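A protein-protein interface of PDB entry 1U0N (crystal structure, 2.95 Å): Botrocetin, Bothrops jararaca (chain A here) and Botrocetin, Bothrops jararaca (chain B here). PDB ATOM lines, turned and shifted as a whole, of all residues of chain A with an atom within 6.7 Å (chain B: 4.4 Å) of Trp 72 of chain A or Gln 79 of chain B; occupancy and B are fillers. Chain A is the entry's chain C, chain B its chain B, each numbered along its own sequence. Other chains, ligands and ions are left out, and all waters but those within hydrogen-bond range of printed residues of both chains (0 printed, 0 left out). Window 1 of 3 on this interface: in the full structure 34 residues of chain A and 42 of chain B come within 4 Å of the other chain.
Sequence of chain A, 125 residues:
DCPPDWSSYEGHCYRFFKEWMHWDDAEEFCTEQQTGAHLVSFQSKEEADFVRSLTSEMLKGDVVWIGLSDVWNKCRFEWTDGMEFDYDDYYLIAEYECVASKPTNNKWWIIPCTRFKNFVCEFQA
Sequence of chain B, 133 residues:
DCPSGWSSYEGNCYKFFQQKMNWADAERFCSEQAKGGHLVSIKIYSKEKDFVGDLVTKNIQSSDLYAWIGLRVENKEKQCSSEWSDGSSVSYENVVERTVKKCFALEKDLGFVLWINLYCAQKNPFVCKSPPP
The backbone carbonyl oxygen (O) of Val 71 of chain A lies within hydrogen-bond range of the backbone NH (N) of Cys 80 of chain B (2.9 Å).
The backbone carbonyl oxygen (O) of Ile 110 of chain A lies within hydrogen-bond range of the side-chain amino group (NZ) of Lys 101 of chain B.
The side-chain carboxylate of Glu 97 of chain A lies within salt-bridge range of the side-chain amino group of Lys 101 of chain B, 2.6 Å away.
The side-chain amide oxygen (OD1) of Asn 117 of chain B sits at hydrogen-bond distance from the backbone NH (N) of Glu 95 of chain A, 2.8 Å away.
SG of Cys 75 of chain A is disulfide-bonded to SG of Cys 80 of chain B, 2.0 Å away.
The backbone NH (N) of Val 71 of chain A is in hydrogen-bond range of the backbone carbonyl oxygen (O) of Glu 97 of chain A.
The backbone carbonyl oxygen of Glu 77 of chain B lies within hydrogen-bond range of the side-chain amino group of Lys 102 of chain B, at 2.8 Å.
OD1 of Asn 73 of chain A is in hydrogen-bond range of N of Ala 94 of chain A (3.3 Å).
The side-chain carboxylate of Glu 97 of chain A lies within hydrogen-bond range of the indole nitrogen of Trp 72 of chain A (2.9 Å).
The side-chain amide nitrogen (NE2) of Gln 79 of chain B lies within hydrogen-bond range of the backbone carbonyl oxygen (O) of Ser 81 of chain B (2.7 Å).
The backbone NH of Val 99 of chain A lies within hydrogen-bond range of the backbone carbonyl oxygen of Leu 68 of chain A.
Of the printed residues of chain B, Leu 68 of chain A touches Gln 79, Ser 81 and Val 90.
Asp 70 of chain A touches none of the printed residues of chain B.
Printed residues of chain B within 4 Å of Trp 72 of chain A: Lys 78, Gln 79, Thr 99, Val 100, Lys 101, Lys 102 and Asn 117.
Printed residues of chain B within 4 Å of Glu 97 of chain A: Lys 101 (2.6 Å).
Printed residues of chain B within 4 Å of Ile 110 of chain A: Gln 79 (3.9 Å), Thr 99 (3.1 Å) and Lys 101 (3.5 Å).
Of the printed residues of chain A, Thr 99 of chain B touches Trp 72 (3.8 Å) and Ile 110 (3.1 Å).
The nearest printed residue of chain B that does not touch Ala 94 of chain A is Lys 101 of chain B (6.3 Å).
Of the 11 printed residues of chain B, 10 touch a printed residue of chain A.
Hydrophobic or aromatic side chains of chain B that line the printed part of chain A: Val 90 and Val 100.
Along chain A the printed residues that touch a printed residue of chain B span positions 68 to 110.
Among the printed residues, 21 pairs touch across the chains.
Among the printed residues, Asp or Glu carboxylates within 4 Å of a Lys or Arg side-chain nitrogen of the other chain: Glu 97 of chain A with Lys 101 of chain B.
Among the printed residues, pairs that only touch across the chains: Trp 72 of chain A with Lys 78 of chain B, Lys 74 of chain A with Cys 80 of chain B, Val 71 of chain A with Gln 79 of chain B, Ile 110 of chain A with Thr 99 of chain B, Trp 72 of chain A with Lys 101 of chain B, Trp 72 of chain A with Asn 117 of chain B, Ala 94 of chain A with Asn 117 of chain B, Leu 68 of chain A with Val 90 of chain B, Trp 72 of chain A with Val 100 of chain B, Leu 68 of chain A with Ser 81 of chain B, Lys 74 of chain A with Ser 81 of chain B, Trp 72 of chain A with Thr 99 of chain B, Ile 110 of chain A with Gln 79 of chain B, Trp 72 of chain A with Lys 102 of chain B, Trp 72 of chain A with Gln 79 of chain B and Leu 68 of chain A with Gln 79 of chain B.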
ATOM      1  N   LEU A  68      -5.316  -9.289 -14.870  1.00  0.00           N
ATOM      2  CA  LEU A  68      -4.834 -10.593 -14.405  1.00  0.00           C
ATOM      3  C   LEU A  68      -4.966 -11.713 -15.437  1.00  0.00           C
ATOM      4  O   LEU A  68      -6.037 -11.906 -16.009  1.00  0.00           O
ATOM      5  CB  LEU A  68      -5.554 -10.971 -13.101  1.00  0.00           C
ATOM      6  CG  LEU A  68      -5.413  -9.952 -11.955  1.00  0.00           C
ATOM      7  CD1 LEU A  68      -6.336 -10.322 -10.808  1.00  0.00           C
ATOM      8  CD2 LEU A  68      -3.957  -9.881 -11.494  1.00  0.00           C
ATOM      9  N   SER A  69      -3.880 -12.454 -15.666  1.00  0.00           N
ATOM     10  CA  SER A  69      -3.892 -13.543 -16.645  1.00  0.00           C
ATOM     11  C   SER A  69      -3.277 -14.871 -16.174  1.00  0.00           C
ATOM     12  O   SER A  69      -2.409 -14.886 -15.305  1.00  0.00           O
ATOM     13  CB  SER A  69      -3.191 -13.095 -17.926  1.00  0.00           C
ATOM     14  OG  SER A  69      -1.826 -12.805 -17.684  1.00  0.00           O
ATOM     15  N   ASP A  70      -3.733 -15.975 -16.770  1.00  0.00           N
ATOM     16  CA  ASP A  70      -3.259 -17.319 -16.426  1.00  0.00           C
ATOM     17  C   ASP A  70      -3.137 -17.477 -14.911  1.00  0.00           C
ATOM     18  O   ASP A  70      -2.058 -17.727 -14.387  1.00  0.00           O
ATOM     19  CB  ASP A  70      -1.898 -17.593 -17.077  1.00  0.00           C
ATOM     20  CG  ASP A  70      -1.534 -19.078 -17.069  1.00  0.00           C
ATOM     21  OD1 ASP A  70      -2.126 -19.834 -16.259  1.00  0.00           O
ATOM     22  OD2 ASP A  70      -0.655 -19.483 -17.867  1.00  0.00           O
ATOM     23  N   VAL A  71      -4.259 -17.355 -14.216  1.00  0.00           N
ATOM     24  CA  VAL A  71      -4.272 -17.434 -12.761  1.00  0.00           C
ATOM     25  C   VAL A  71      -4.247 -18.804 -12.095  1.00  0.00           C
ATOM     26  O   VAL A  71      -4.342 -18.880 -10.878  1.00  0.00           O
ATOM     27  CB  VAL A  71      -5.483 -16.670 -12.197  1.00  0.00           C
ATOM     28  CG1 VAL A  71      -5.518 -15.255 -12.789  1.00  0.00           C
ATOM     29  CG2 VAL A  71      -6.781 -17.438 -12.498  1.00  0.00           C
ATOM     30  N   TRP A  72      -4.127 -19.881 -12.865  1.00  0.00           N
ATOM     31  CA  TRP A  72      -4.089 -21.224 -12.276  1.00  0.00           C
ATOM     32  C   TRP A  72      -2.720 -21.890 -12.436  1.00  0.00           C
ATOM     33  O   TRP A  72      -2.315 -22.714 -11.617  1.00  0.00           O
ATOM     34  CB  TRP A  72      -5.188 -22.113 -12.882  1.00  0.00           C
ATOM     35  CG  TRP A  72      -6.559 -21.634 -12.549  1.00  0.00           C
ATOM     36  CD1 TRP A  72      -7.629 -21.515 -13.401  1.00  0.00           C
ATOM     37  CD2 TRP A  72      -7.002 -21.134 -11.282  1.00  0.00           C
ATOM     38  NE1 TRP A  72      -8.705 -20.963 -12.741  1.00  0.00           N
ATOM     39  CE2 TRP A  72      -8.347 -20.719 -11.440  1.00  0.00           C
ATOM     40  CE3 TRP A  72      -6.392 -20.994 -10.025  1.00  0.00           C
ATOM     41  CZ2 TRP A  72      -9.087 -20.172 -10.391  1.00  0.00           C
ATOM     42  CZ3 TRP A  72      -7.132 -20.450  -8.982  1.00  0.00           C
ATOM     43  CH2 TRP A  72      -8.465 -20.046  -9.174  1.00  0.00           C
ATOM     44  N   ASN A  73      -1.994 -21.534 -13.482  1.00  0.00           N
ATOM     45  CA  ASN A  73      -0.694 -22.135 -13.675  1.00  0.00           C
ATOM     46  C   ASN A  73       0.355 -21.414 -12.847  1.00  0.00           C
ATOM     47  O   ASN A  73       1.389 -21.993 -12.493  1.00  0.00           O
ATOM     48  CB  ASN A  73      -0.332 -22.135 -15.155  1.00  0.00           C
ATOM     49  CG  ASN A  73      -1.193 -23.096 -15.948  1.00  0.00           C
ATOM     50  OD1 ASN A  73      -1.176 -24.302 -15.701  1.00  0.00           O
ATOM     51  ND2 ASN A  73      -1.969 -22.565 -16.895  1.00  0.00           N
ATOM     52  N   LYS A  74       0.083 -20.158 -12.514  1.00  0.00           N
ATOM     53  CA  LYS A  74       1.020 -19.392 -11.701  1.00  0.00           C
ATOM     54  C   LYS A  74       0.998 -19.917 -10.261  1.00  0.00           C
ATOM     55  O   LYS A  74       1.790 -19.496  -9.413  1.00  0.00           O
ATOM     56  CB  LYS A  74       0.654 -17.909 -11.756  1.00  0.00           C
ATOM     57  CG  LYS A  74       0.778 -17.356 -13.147  1.00  0.00           C
ATOM     58  CD  LYS A  74       0.328 -15.922 -13.241  1.00  0.00           C
ATOM     59  CE  LYS A  74       0.440 -15.422 -14.681  1.00  0.00           C
ATOM     60  NZ  LYS A  74       0.073 -13.984 -14.803  1.00  0.00           N
ATOM     61  N   CYS A  75       0.102 -20.870 -10.011  1.00  0.00           N
ATOM     62  CA  CYS A  75      -0.064 -21.465  -8.691  1.00  0.00           C
ATOM     63  C   CYS A  75       1.050 -22.421  -8.243  1.00  0.00           C
ATOM     64  O   CYS A  75       1.925 -22.789  -9.026  1.00  0.00           O
ATOM     65  CB  CYS A  75      -1.399 -22.203  -8.633  1.00  0.00           C
ATOM     66  SG  CYS A  75      -2.856 -21.201  -9.055  1.00  0.00           S
ATOM     67  N   ARG A  76       0.982 -22.814  -6.973  1.00  0.00           N
ATOM     68  CA  ARG A  76       1.927 -23.733  -6.336  1.00  0.00           C
ATOM     69  C   ARG A  76       1.055 -24.904  -5.893  1.00  0.00           C
ATOM     70  O   ARG A  76       0.213 -24.744  -5.012  1.00  0.00           O
ATOM     71  CB  ARG A  76       2.530 -23.062  -5.107  1.00  0.00           C
ATOM     72  CG  ARG A  76       3.938 -23.472  -4.743  1.00  0.00           C
ATOM     73  CD  ARG A  76       4.559 -22.382  -3.870  1.00  0.00           C
ATOM     74  NE  ARG A  76       6.018 -22.394  -3.922  1.00  0.00           N
ATOM     75  CZ  ARG A  76       6.732 -22.307  -5.041  1.00  0.00           C
ATOM     76  NH1 ARG A  76       6.123 -22.203  -6.211  1.00  0.00           N
ATOM     77  NH2 ARG A  76       8.058 -22.331  -4.990  1.00  0.00           N
ATOM     78  N   PHE A  77       1.251 -26.075  -6.488  1.00  0.00           N
ATOM     79  CA  PHE A  77       0.423 -27.242  -6.174  1.00  0.00           C
ATOM     80  C   PHE A  77       0.973 -28.169  -5.097  1.00  0.00           C
ATOM     81  O   PHE A  77       2.136 -28.095  -4.746  1.00  0.00           O
ATOM     82  CB  PHE A  77       0.183 -28.050  -7.459  1.00  0.00           C
ATOM     83  CG  PHE A  77      -0.241 -27.207  -8.631  1.00  0.00           C
ATOM     84  CD1 PHE A  77       0.668 -26.869  -9.626  1.00  0.00           C
ATOM     85  CD2 PHE A  77      -1.542 -26.717  -8.720  1.00  0.00           C
ATOM     86  CE1 PHE A  77       0.286 -26.051 -10.688  1.00  0.00           C
ATOM     87  CE2 PHE A  77      -1.926 -25.898  -9.779  1.00  0.00           C
ATOM     88  CZ  PHE A  77      -1.011 -25.567 -10.764  1.00  0.00           C
ATOM     89  N   ILE A  93      -0.838 -27.878 -16.822  1.00  0.00           N
ATOM     90  CA  ILE A  93      -1.861 -28.805 -16.317  1.00  0.00           C
ATOM     91  C   ILE A  93      -3.139 -28.206 -15.742  1.00  0.00           C
ATOM     92  O   ILE A  93      -4.135 -28.914 -15.584  1.00  0.00           O
ATOM     93  CB  ILE A  93      -1.288 -29.861 -15.286  1.00  0.00           C
ATOM     94  CG1 ILE A  93      -1.594 -29.473 -13.833  1.00  0.00           C
ATOM     95  CG2 ILE A  93       0.170 -30.072 -15.534  1.00  0.00           C
ATOM     96  CD1 ILE A  93      -0.708 -28.443 -13.232  1.00  0.00           C
ATOM     97  N   ALA A  94      -3.127 -26.914 -15.442  1.00  0.00           N
ATOM     98  CA  ALA A  94      -4.319 -26.276 -14.908  1.00  0.00           C
ATOM     99  C   ALA A  94      -4.979 -25.519 -16.043  1.00  0.00           C
ATOM    100  O   ALA A  94      -4.328 -25.233 -17.041  1.00  0.00           O
ATOM    101  CB  ALA A  94      -3.944 -25.332 -13.801  1.00  0.00           C
ATOM    102  N   GLU A  95      -6.263 -25.197 -15.896  1.00  0.00           N
ATOM    103  CA  GLU A  95      -6.999 -24.469 -16.929  1.00  0.00           C
ATOM    104  C   GLU A  95      -6.371 -23.110 -17.206  1.00  0.00           C
ATOM    105  O   GLU A  95      -5.974 -22.400 -16.283  1.00  0.00           O
ATOM    106  CB  GLU A  95      -8.447 -24.263 -16.496  1.00  0.00           C
ATOM    107  CG  GLU A  95      -9.197 -25.536 -16.262  1.00  0.00           C
ATOM    108  CD  GLU A  95     -10.277 -25.769 -17.297  1.00  0.00           C
ATOM    109  OE1 GLU A  95     -10.005 -25.512 -18.491  1.00  0.00           O
ATOM    110  OE2 GLU A  95     -11.388 -26.218 -16.911  1.00  0.00           O
ATOM    111  N   TYR A  96      -6.296 -22.735 -18.475  1.00  0.00           N
ATOM    112  CA  TYR A  96      -5.710 -21.452 -18.833  1.00  0.00           C
ATOM    113  C   TYR A  96      -6.780 -20.379 -18.866  1.00  0.00           C
ATOM    114  O   TYR A  96      -7.445 -20.191 -19.876  1.00  0.00           O
ATOM    115  CB  TYR A  96      -5.027 -21.543 -20.196  1.00  0.00           C
ATOM    116  CG  TYR A  96      -4.186 -20.339 -20.555  1.00  0.00           C
ATOM    117  CD1 TYR A  96      -4.702 -19.306 -21.337  1.00  0.00           C
ATOM    118  CD2 TYR A  96      -2.865 -20.246 -20.127  1.00  0.00           C
ATOM    119  CE1 TYR A  96      -3.914 -18.210 -21.689  1.00  0.00           C
ATOM    120  CE2 TYR A  96      -2.073 -19.160 -20.467  1.00  0.00           C
ATOM    121  CZ  TYR A  96      -2.595 -18.146 -21.247  1.00  0.00           C
ATOM    122  OH  TYR A  96      -1.785 -17.075 -21.586  1.00  0.00           O
ATOM    123  N   GLU A  97      -6.940 -19.667 -17.758  1.00  0.00           N
ATOM    124  CA  GLU A  97      -7.950 -18.624 -17.678  1.00  0.00           C
ATOM    125  C   GLU A  97      -7.452 -17.253 -17.182  1.00  0.00           C
ATOM    126  O   GLU A  97      -6.416 -17.113 -16.517  1.00  0.00           O
ATOM    127  CB  GLU A  97      -9.085 -19.118 -16.801  1.00  0.00           C
ATOM    128  CG  GLU A  97      -9.243 -20.607 -16.890  1.00  0.00           C
ATOM    129  CD  GLU A  97     -10.445 -21.104 -16.150  1.00  0.00           C
ATOM    130  OE1 GLU A  97     -10.566 -20.802 -14.941  1.00  0.00           O
ATOM    131  OE2 GLU A  97     -11.264 -21.799 -16.785  1.00  0.00           O
ATOM    132  N   VAL A  99      -8.904 -13.167 -15.771  1.00  0.00           N
ATOM    133  CA  VAL A  99      -9.965 -12.540 -14.979  1.00  0.00           C
ATOM    134  C   VAL A  99     -10.684 -11.424 -15.738  1.00  0.00           C
ATOM    135  O   VAL A  99     -10.068 -10.658 -16.474  1.00  0.00           O
ATOM    136  CB  VAL A  99      -9.401 -11.952 -13.658  1.00  0.00           C
ATOM    137  CG1 VAL A  99     -10.525 -11.390 -12.820  1.00  0.00           C
ATOM    138  CG2 VAL A  99      -8.654 -13.019 -12.880  1.00  0.00           C
ATOM    139  N   TRP A 108     -15.685  -9.882 -10.241  1.00  0.00           N
ATOM    140  CA  TRP A 108     -14.738 -10.507 -11.159  1.00  0.00           C
ATOM    141  C   TRP A 108     -15.086 -11.944 -11.534  1.00  0.00           C
ATOM    142  O   TRP A 108     -15.704 -12.671 -10.760  1.00  0.00           O
ATOM    143  CB  TRP A 108     -13.337 -10.476 -10.550  1.00  0.00           C
ATOM    144  CG  TRP A 108     -12.843  -9.096 -10.210  1.00  0.00           C
ATOM    145  CD1 TRP A 108     -13.496  -7.910 -10.413  1.00  0.00           C
ATOM    146  CD2 TRP A 108     -11.573  -8.761  -9.633  1.00  0.00           C
ATOM    147  NE1 TRP A 108     -12.709  -6.860 -10.002  1.00  0.00           N
ATOM    148  CE2 TRP A 108     -11.523  -7.353  -9.520  1.00  0.00           C
ATOM    149  CE3 TRP A 108     -10.470  -9.514  -9.204  1.00  0.00           C
ATOM    150  CZ2 TRP A 108     -10.412  -6.683  -8.996  1.00  0.00           C
ATOM    151  CZ3 TRP A 108      -9.369  -8.847  -8.685  1.00  0.00           C
ATOM    152  CH2 TRP A 108      -9.349  -7.445  -8.586  1.00  0.00           C
ATOM    153  N   ILE A 110     -13.271 -15.440 -13.307  1.00  0.00           N
ATOM    154  CA  ILE A 110     -12.122 -16.124 -13.856  1.00  0.00           C
ATOM    155  C   ILE A 110     -12.703 -17.051 -14.927  1.00  0.00           C
ATOM    156  O   ILE A 110     -13.434 -18.003 -14.627  1.00  0.00           O
ATOM    157  CB  ILE A 110     -11.375 -16.901 -12.750  1.00  0.00           C
ATOM    158  CG1 ILE A 110     -11.044 -15.943 -11.602  1.00  0.00           C
ATOM    159  CG2 ILE A 110     -10.105 -17.519 -13.306  1.00  0.00           C
ATOM    160  CD1 ILE A 110     -10.368 -16.585 -10.426  1.00  0.00           C
ATOM    161  N   ILE A 111     -12.389 -16.737 -16.182  1.00  0.00           N
ATOM    162  CA  ILE A 111     -12.889 -17.483 -17.328  1.00  0.00           C
ATOM    163  C   ILE A 111     -11.760 -17.769 -18.330  1.00  0.00           C
ATOM    164  O   ILE A 111     -10.691 -17.159 -18.253  1.00  0.00           O
ATOM    165  CB  ILE A 111     -13.989 -16.661 -18.001  1.00  0.00           C
ATOM    166  CG1 ILE A 111     -13.400 -15.351 -18.540  1.00  0.00           C
ATOM    167  CG2 ILE A 111     -15.051 -16.313 -16.976  1.00  0.00           C
ATOM    168  CD1 ILE A 111     -14.400 -14.442 -19.218  1.00  0.00           C
ATOM    169  N   GLU B  77      -4.604 -17.583  -1.875  1.00  0.00           N
ATOM    170  CA  GLU B  77      -5.422 -16.659  -2.657  1.00  0.00           C
ATOM    171  C   GLU B  77      -6.527 -17.362  -3.442  1.00  0.00           C
ATOM    172  O   GLU B  77      -6.582 -18.587  -3.511  1.00  0.00           O
ATOM    173  CB  GLU B  77      -4.544 -15.863  -3.625  1.00  0.00           C
ATOM    174  CG  GLU B  77      -3.570 -14.905  -2.956  1.00  0.00           C
ATOM    175  CD  GLU B  77      -2.749 -15.573  -1.865  1.00  0.00           C
ATOM    176  OE1 GLU B  77      -2.190 -16.663  -2.118  1.00  0.00           O
ATOM    177  OE2 GLU B  77      -2.660 -15.004  -0.755  1.00  0.00           O
ATOM    178  N   LYS B  78      -7.416 -16.569  -4.025  1.00  0.00           N
ATOM    179  CA  LYS B  78      -8.501 -17.115  -4.817  1.00  0.00           C
ATOM    180  C   LYS B  78      -7.933 -17.430  -6.189  1.00  0.00           C
ATOM    181  O   LYS B  78      -8.326 -18.403  -6.821  1.00  0.00           O
ATOM    182  CB  LYS B  78      -9.638 -16.099  -4.952  1.00  0.00           C
ATOM    183  CG  LYS B  78     -10.298 -15.709  -3.642  1.00  0.00           C
ATOM    184  CD  LYS B  78     -11.424 -14.707  -3.867  1.00  0.00           C
ATOM    185  CE  LYS B  78     -12.059 -14.284  -2.549  1.00  0.00           C
ATOM    186  NZ  LYS B  78     -12.635 -15.452  -1.823  1.00  0.00           N
ATOM    187  N   GLN B  79      -7.013 -16.584  -6.643  1.00  0.00           N
ATOM    188  CA  GLN B  79      -6.356 -16.749  -7.938  1.00  0.00           C
ATOM    189  C   GLN B  79      -4.861 -16.580  -7.707  1.00  0.00           C
ATOM    190  O   GLN B  79      -4.468 -15.946  -6.743  1.00  0.00           O
ATOM    191  CB  GLN B  79      -6.896 -15.724  -8.943  1.00  0.00           C
ATOM    192  CG  GLN B  79      -6.712 -14.267  -8.567  1.00  0.00           C
ATOM    193  CD  GLN B  79      -5.366 -13.728  -8.992  1.00  0.00           C
ATOM    194  OE1 GLN B  79      -4.895 -14.019 -10.087  1.00  0.00           O
ATOM    195  NE2 GLN B  79      -4.746 -12.925  -8.135  1.00  0.00           N
ATOM    196  N   CYS B  80      -4.020 -17.139  -8.567  1.00  0.00           N
ATOM    197  CA  CYS B  80      -2.593 -17.037  -8.320  1.00  0.00           C
ATOM    198  C   CYS B  80      -1.813 -16.021  -9.121  1.00  0.00           C
ATOM    199  O   CYS B  80      -0.724 -16.316  -9.609  1.00  0.00           O
ATOM    200  CB  CYS B  80      -1.928 -18.399  -8.479  1.00  0.00           C
ATOM    201  SG  CYS B  80      -2.838 -19.734  -7.654  1.00  0.00           S
ATOM    202  N   SER B  81      -2.353 -14.826  -9.274  1.00  0.00           N
ATOM    203  CA  SER B  81      -1.612 -13.806  -9.987  1.00  0.00           C
ATOM    204  C   SER B  81      -1.393 -12.702  -8.958  1.00  0.00           C
ATOM    205  O   SER B  81      -2.301 -11.921  -8.661  1.00  0.00           O
ATOM    206  CB  SER B  81      -2.398 -13.294 -11.189  1.00  0.00           C
ATOM    207  OG  SER B  81      -1.578 -12.474 -12.000  1.00  0.00           O
ATOM    208  N   VAL B  90      -1.410  -7.066  -6.554  1.00  0.00           N
ATOM    209  CA  VAL B  90      -2.817  -7.316  -6.263  1.00  0.00           C
ATOM    210  C   VAL B  90      -3.101  -7.315  -4.767  1.00  0.00           C
ATOM    211  O   VAL B  90      -2.516  -8.089  -4.010  1.00  0.00           O
ATOM    212  CB  VAL B  90      -3.277  -8.671  -6.858  1.00  0.00           C
ATOM    213  CG1 VAL B  90      -4.571  -9.141  -6.184  1.00  0.00           C
ATOM    214  CG2 VAL B  90      -3.486  -8.520  -8.362  1.00  0.00           C
ATOM    215  N   THR B  99     -15.833 -19.883  -9.079  1.00  0.00           N
ATOM    216  CA  THR B  99     -15.093 -19.636 -10.302  1.00  0.00           C
ATOM    217  C   THR B  99     -13.652 -20.012  -9.995  1.00  0.00           C
ATOM    218  O   THR B  99     -12.828 -20.204 -10.886  1.00  0.00           O
ATOM    219  CB  THR B  99     -15.227 -18.140 -10.687  1.00  0.00           C
ATOM    220  OG1 THR B  99     -16.254 -17.998 -11.670  1.00  0.00           O
ATOM    221  CG2 THR B  99     -13.948 -17.570 -11.215  1.00  0.00           C
ATOM    222  N   VAL B 100     -13.361 -20.123  -8.706  1.00  0.00           N
ATOM    223  CA  VAL B 100     -12.039 -20.505  -8.258  1.00  0.00           C
ATOM    224  C   VAL B 100     -11.961 -22.027  -8.382  1.00  0.00           C
ATOM    225  O   VAL B 100     -12.697 -22.759  -7.715  1.00  0.00           O
ATOM    226  CB  VAL B 100     -11.808 -20.098  -6.790  1.00  0.00           C
ATOM    227  CG1 VAL B 100     -10.449 -20.546  -6.350  1.00  0.00           C
ATOM    228  CG2 VAL B 100     -11.930 -18.595  -6.637  1.00  0.00           C
ATOM    229  N   LYS B 101     -11.077 -22.489  -9.260  1.00  0.00           N
ATOM    230  CA  LYS B 101     -10.878 -23.909  -9.504  1.00  0.00           C
ATOM    231  C   LYS B 101      -9.542 -24.301  -8.875  1.00  0.00           C
ATOM    232  O   LYS B 101      -8.508 -24.266  -9.540  1.00  0.00           O
ATOM    233  CB  LYS B 101     -10.847 -24.150 -11.010  1.00  0.00           C
ATOM    234  CG  LYS B 101     -11.963 -23.446 -11.752  1.00  0.00           C
ATOM    235  CD  LYS B 101     -11.852 -23.650 -13.249  1.00  0.00           C
ATOM    236  CE  LYS B 101     -12.915 -22.855 -14.013  1.00  0.00           C
ATOM    237  NZ  LYS B 101     -12.818 -21.356 -13.878  1.00  0.00           N
ATOM    238  N   LYS B 102      -9.567 -24.685  -7.598  1.00  0.00           N
ATOM    239  CA  LYS B 102      -8.340 -25.042  -6.885  1.00  0.00           C
ATOM    240  C   LYS B 102      -8.152 -26.498  -6.490  1.00  0.00           C
ATOM    241  O   LYS B 102      -7.267 -26.801  -5.693  1.00  0.00           O
ATOM    242  CB  LYS B 102      -8.200 -24.164  -5.636  1.00  0.00           C
ATOM    243  CG  LYS B 102      -8.075 -22.678  -5.955  1.00  0.00           C
ATOM    244  CD  LYS B 102      -8.208 -21.795  -4.732  1.00  0.00           C
ATOM    245  CE  LYS B 102      -7.095 -22.014  -3.744  1.00  0.00           C
ATOM    246  NZ  LYS B 102      -7.324 -21.148  -2.557  1.00  0.00           N
ATOM    247  N   ASN B 117      -8.553 -28.888 -13.092  1.00  0.00           N
ATOM    248  CA  ASN B 117      -8.917 -28.220 -11.845  1.00  0.00           C
ATOM    249  C   ASN B 117     -10.366 -27.740 -11.893  1.00  0.00           C
ATOM    250  O   ASN B 117     -10.829 -27.202 -12.904  1.00  0.00           O
ATOM    251  CB  ASN B 117      -7.948 -27.068 -11.506  1.00  0.00           C
ATOM    252  CG  ASN B 117      -7.624 -26.186 -12.692  1.00  0.00           C
ATOM    253  OD1 ASN B 117      -7.553 -26.649 -13.823  1.00  0.00           O
ATOM    254  ND2 ASN B 117      -7.387 -24.911 -12.427  1.00  0.00           N
